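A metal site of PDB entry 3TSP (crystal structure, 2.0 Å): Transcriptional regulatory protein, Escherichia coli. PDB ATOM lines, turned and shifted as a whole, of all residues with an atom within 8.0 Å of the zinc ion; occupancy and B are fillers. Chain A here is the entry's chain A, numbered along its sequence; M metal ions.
O of Cys 45 sits at hydrogen-bond distance from NH1 of Arg 48. The guanidinium group (NH2) of Arg 83 sits close to the side-chain sulfur (SG) of Cys 23, at 3.3 Å. NE of Arg 83 lies close to SG of Cys 42. SG of Cys 42 lies close to N of His 44 (3.3 Å). The guanidinium group (NH1) of Arg 48 lies within hydrogen-bond range of the backbone carbonyl oxygen (O) of Cys 42, at 3.2 Å.
Within 4 Å of the zinc ion: Cys 20, Cys 23, Cys 42 and Cys 45.
SG of Cys 45 is bound to the zinc ion. The side-chain sulfur (SG) of Cys 23 is bound to the zinc ion (2.3 Å). The side-chain sulfur (SG) of Cys 20 is bound to the zinc ion, 2.4 Å away. The side-chain sulfur (SG) of Cys 42 binds the zinc ion (2.4 Å). The zinc ion has four donor atoms within binding distance.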
ATOM      1  N   ALA A  17       2.444  28.587  -5.915  1.00  0.00           N
ATOM      2  CA  ALA A  17       3.447  27.514  -5.946  1.00  0.00           C
ATOM      3  C   ALA A  17       3.003  26.267  -5.197  1.00  0.00           C
ATOM      4  O   ALA A  17       2.404  26.353  -4.140  1.00  0.00           O
ATOM      5  CB  ALA A  17       4.830  28.004  -5.435  1.00  0.00           C
ATOM      6  N   ALA A  18       3.333  25.096  -5.764  1.00  0.00           N
ATOM      7  CA  ALA A  18       3.021  23.795  -5.186  1.00  0.00           C
ATOM      8  C   ALA A  18       3.602  23.683  -3.801  1.00  0.00           C
ATOM      9  O   ALA A  18       4.755  24.109  -3.582  1.00  0.00           O
ATOM     10  CB  ALA A  18       3.618  22.692  -6.082  1.00  0.00           C
ATOM     11  N   THR A  19       2.841  23.131  -2.861  1.00  0.00           N
ATOM     12  CA  THR A  19       3.372  22.833  -1.516  1.00  0.00           C
ATOM     13  C   THR A  19       4.791  22.200  -1.598  1.00  0.00           C
ATOM     14  O   THR A  19       4.997  21.200  -2.323  1.00  0.00           O
ATOM     15  CB  THR A  19       2.387  21.914  -0.726  1.00  0.00           C
ATOM     16  OG1 THR A  19       1.092  22.542  -0.695  1.00  0.00           O
ATOM     17  CG2 THR A  19       2.878  21.677   0.740  1.00  0.00           C
ATOM     18  N   CYS A  20       5.756  22.760  -0.857  1.00  0.00           N
ATOM     19  CA  CYS A  20       7.137  22.274  -0.928  1.00  0.00           C
ATOM     20  C   CYS A  20       7.345  20.982  -0.100  1.00  0.00           C
ATOM     21  O   CYS A  20       6.479  20.587   0.716  1.00  0.00           O
ATOM     22  CB  CYS A  20       8.138  23.380  -0.518  1.00  0.00           C
ATOM     23  SG  CYS A  20       8.089  23.748   1.273  1.00  0.00           S
ATOM     24  N   PRO A  21       8.482  20.294  -0.328  1.00  0.00           N
ATOM     25  CA  PRO A  21       8.763  19.082   0.482  1.00  0.00           C
ATOM     26  C   PRO A  21       8.828  19.331   1.993  1.00  0.00           C
ATOM     27  O   PRO A  21       8.259  18.562   2.761  1.00  0.00           O
ATOM     28  CB  PRO A  21      10.099  18.574  -0.081  1.00  0.00           C
ATOM     29  CG  PRO A  21      10.111  19.150  -1.536  1.00  0.00           C
ATOM     30  CD  PRO A  21       9.505  20.519  -1.378  1.00  0.00           C
ATOM     31  N   ALA A  22       9.497  20.396   2.417  1.00  0.00           N
ATOM     32  CA  ALA A  22       9.525  20.778   3.834  1.00  0.00           C
ATOM     33  C   ALA A  22       8.129  21.028   4.430  1.00  0.00           C
ATOM     34  O   ALA A  22       7.862  20.578   5.519  1.00  0.00           O
ATOM     35  CB  ALA A  22      10.457  22.010   4.035  1.00  0.00           C
ATOM     36  N   CYS A  23       7.227  21.733   3.745  1.00  0.00           N
ATOM     37  CA  CYS A  23       5.860  21.887   4.253  1.00  0.00           C
ATOM     38  C   CYS A  23       5.098  20.559   4.262  1.00  0.00           C
ATOM     39  O   CYS A  23       4.292  20.293   5.159  1.00  0.00           O
ATOM     40  CB  CYS A  23       5.079  22.943   3.459  1.00  0.00           C
ATOM     41  SG  CYS A  23       5.461  24.641   3.900  1.00  0.00           S
ATOM     42  N   LEU A  24       5.331  19.732   3.258  1.00  0.00           N
ATOM     43  CA  LEU A  24       4.665  18.422   3.188  1.00  0.00           C
ATOM     44  C   LEU A  24       5.121  17.531   4.349  1.00  0.00           C
ATOM     45  O   LEU A  24       4.317  16.879   4.995  1.00  0.00           O
ATOM     46  CB  LEU A  24       4.907  17.757   1.818  1.00  0.00           C
ATOM     47  CG  LEU A  24       4.148  16.436   1.588  1.00  0.00           C
ATOM     48  CD1 LEU A  24       2.645  16.599   1.779  1.00  0.00           C
ATOM     49  CD2 LEU A  24       4.451  15.850   0.236  1.00  0.00           C
ATOM     50  N   GLU A  26       6.396  18.673   7.302  1.00  0.00           N
ATOM     51  CA  GLU A  26       5.824  19.248   8.533  1.00  0.00           C
ATOM     52  C   GLU A  26       4.358  18.794   8.736  1.00  0.00           C
ATOM     53  O   GLU A  26       3.988  18.386   9.833  1.00  0.00           O
ATOM     54  CB  GLU A  26       5.947  20.770   8.502  1.00  0.00           C
ATOM     55  CG  GLU A  26       5.439  21.503   9.737  1.00  0.00           C
ATOM     56  CD  GLU A  26       5.579  23.003   9.627  1.00  0.00           C
ATOM     57  OE1 GLU A  26       6.318  23.520   8.722  1.00  0.00           O
ATOM     58  OE2 GLU A  26       4.927  23.708  10.445  1.00  0.00           O
ATOM     59  N   ILE A  40      -1.128  24.807   5.366  1.00  0.00           N
ATOM     60  CA  ILE A  40       0.296  24.988   5.593  1.00  0.00           C
ATOM     61  C   ILE A  40       0.961  25.551   4.327  1.00  0.00           C
ATOM     62  O   ILE A  40       0.663  25.123   3.182  1.00  0.00           O
ATOM     63  CB  ILE A  40       0.959  23.655   6.029  1.00  0.00           C
ATOM     64  CG1 ILE A  40       2.431  23.875   6.402  1.00  0.00           C
ATOM     65  CG2 ILE A  40       0.812  22.559   4.939  1.00  0.00           C
ATOM     66  CD1 ILE A  40       3.014  22.674   7.193  1.00  0.00           C
ATOM     67  N   ASN A  41       1.807  26.562   4.548  1.00  0.00           N
ATOM     68  CA  ASN A  41       2.651  27.145   3.470  1.00  0.00           C
ATOM     69  C   ASN A  41       3.869  27.769   4.114  1.00  0.00           C
ATOM     70  O   ASN A  41       3.923  27.894   5.336  1.00  0.00           O
ATOM     71  CB  ASN A  41       1.889  28.183   2.610  1.00  0.00           C
ATOM     72  CG  ASN A  41       1.216  29.274   3.431  1.00  0.00           C
ATOM     73  OD1 ASN A  41       0.002  29.243   3.634  1.00  0.00           O
ATOM     74  ND2 ASN A  41       1.981  30.265   3.903  1.00  0.00           N
ATOM     75  N   CYS A  42       4.842  28.124   3.312  1.00  0.00           N
ATOM     76  CA  CYS A  42       6.009  28.832   3.825  1.00  0.00           C
ATOM     77  C   CYS A  42       6.463  29.879   2.819  1.00  0.00           C
ATOM     78  O   CYS A  42       5.774  30.180   1.862  1.00  0.00           O
ATOM     79  CB  CYS A  42       7.140  27.844   4.150  1.00  0.00           C
ATOM     80  SG  CYS A  42       7.950  27.146   2.696  1.00  0.00           S
ATOM     81  N   THR A  43       7.641  30.433   3.038  1.00  0.00           N
ATOM     82  CA  THR A  43       8.120  31.474   2.156  1.00  0.00           C
ATOM     83  C   THR A  43       8.374  30.959   0.733  1.00  0.00           C
ATOM     84  O   THR A  43       8.343  31.740  -0.226  1.00  0.00           O
ATOM     85  CB  THR A  43       9.334  32.229   2.764  1.00  0.00           C
ATOM     86  OG1 THR A  43       9.494  33.470   2.076  1.00  0.00           O
ATOM     87  CG2 THR A  43      10.641  31.395   2.683  1.00  0.00           C
ATOM     88  N   HIS A  44       8.553  29.646   0.594  1.00  0.00           N
ATOM     89  CA  HIS A  44       8.800  28.984  -0.699  1.00  0.00           C
ATOM     90  C   HIS A  44       7.580  28.437  -1.432  1.00  0.00           C
ATOM     91  O   HIS A  44       7.693  28.064  -2.603  1.00  0.00           O
ATOM     92  CB  HIS A  44       9.853  27.890  -0.541  1.00  0.00           C
ATOM     93  CG  HIS A  44      11.137  28.407   0.046  1.00  0.00           C
ATOM     94  ND1 HIS A  44      11.582  28.040   1.295  1.00  0.00           N
ATOM     95  CD2 HIS A  44      12.032  29.304  -0.436  1.00  0.00           C
ATOM     96  CE1 HIS A  44      12.720  28.670   1.542  1.00  0.00           C
ATOM     97  NE2 HIS A  44      13.011  29.450   0.512  1.00  0.00           N
ATOM     98  N   CYS A  45       6.429  28.350  -0.782  1.00  0.00           N
ATOM     99  CA  CYS A  45       5.303  27.714  -1.430  1.00  0.00           C
ATOM    100  C   CYS A  45       3.985  28.329  -1.004  1.00  0.00           C
ATOM    101  O   CYS A  45       3.939  29.154  -0.087  1.00  0.00           O
ATOM    102  CB  CYS A  45       5.297  26.197  -1.169  1.00  0.00           C
ATOM    103  SG  CYS A  45       4.790  25.738   0.453  1.00  0.00           S
ATOM    104  N   GLY A  46       2.904  27.915  -1.672  1.00  0.00           N
ATOM    105  CA  GLY A  46       1.614  28.360  -1.254  1.00  0.00           C
ATOM    106  C   GLY A  46       1.030  29.335  -2.265  1.00  0.00           C
ATOM    107  O   GLY A  46       1.659  29.657  -3.267  1.00  0.00           O
ATOM    108  N   ARG A  48      -0.222  32.717  -4.047  1.00  0.00           N
ATOM    109  CA  ARG A  48       0.370  34.057  -4.189  1.00  0.00           C
ATOM    110  C   ARG A  48      -0.646  34.988  -4.869  1.00  0.00           C
ATOM    111  O   ARG A  48      -1.476  35.623  -4.193  1.00  0.00           O
ATOM    112  CB  ARG A  48       1.685  33.955  -4.994  1.00  0.00           C
ATOM    113  CG  ARG A  48       2.778  33.175  -4.293  1.00  0.00           C
ATOM    114  CD  ARG A  48       3.343  33.952  -3.093  1.00  0.00           C
ATOM    115  NE  ARG A  48       4.435  33.232  -2.434  1.00  0.00           N
ATOM    116  CZ  ARG A  48       4.283  32.349  -1.452  1.00  0.00           C
ATOM    117  NH1 ARG A  48       5.349  31.750  -0.938  1.00  0.00           N
ATOM    118  NH2 ARG A  48       3.056  32.024  -0.989  1.00  0.00           N
ATOM    119  N   ARG A  83      11.929  29.258   7.997  1.00  0.00           N
ATOM    120  CA  ARG A  83      11.416  29.022   6.647  1.00  0.00           C
ATOM    121  C   ARG A  83      10.111  29.785   6.360  1.00  0.00           C
ATOM    122  O   ARG A  83       9.762  29.999   5.193  1.00  0.00           O
ATOM    123  CB  ARG A  83      11.213  27.518   6.385  1.00  0.00           C
ATOM    124  CG  ARG A  83      11.010  27.215   4.885  1.00  0.00           C
ATOM    125  CD  ARG A  83      10.819  25.746   4.590  1.00  0.00           C
ATOM    126  NE  ARG A  83       9.474  25.295   4.888  1.00  0.00           N
ATOM    127  CZ  ARG A  83       9.110  24.637   5.994  1.00  0.00           C
ATOM    128  NH1 ARG A  83       9.979  24.348   6.938  1.00  0.00           N
ATOM    129  NH2 ARG A  83       7.852  24.256   6.135  1.00  0.00           N
ATOM    130  N   ARG A  84       9.422  30.202   7.423  1.00  0.00           N
ATOM    131  CA  ARG A  84       8.170  30.946   7.293  1.00  0.00           C
ATOM    132  C   ARG A  84       8.341  32.461   7.500  1.00  0.00           C
ATOM    133  O   ARG A  84       7.347  33.192   7.636  1.00  0.00           O
ATOM    134  CB  ARG A  84       7.102  30.380   8.230  1.00  0.00           C
ATOM    135  CG  ARG A  84       6.726  28.961   7.843  1.00  0.00           C
ATOM    136  CD  ARG A  84       6.186  28.197   9.012  1.00  0.00           C
ATOM    137  NE  ARG A  84       6.787  26.856   9.141  1.00  0.00           N
ATOM    138  CZ  ARG A  84       7.783  26.537   9.990  1.00  0.00           C
ATOM    139  NH1 ARG A  84       8.333  27.445  10.795  1.00  0.00           N
ATOM    140  NH2 ARG A  84       8.227  25.280  10.022  1.00  0.00           N
ATOM    141  N   ALA A  87       6.213  34.717   5.514  1.00  0.00           N
ATOM    142  CA  ALA A  87       5.288  33.916   4.703  1.00  0.00           C
ATOM    143  C   ALA A  87       3.917  34.596   4.880  1.00  0.00           C
ATOM    144  O   ALA A  87       3.258  34.429   5.927  1.00  0.00           O
ATOM    145  CB  ALA A  87       5.266  32.463   5.156  1.00  0.00           C
HETATM  146 ZN    ZN M   1       6.531  25.384   1.956  1.00  0.00          ZN
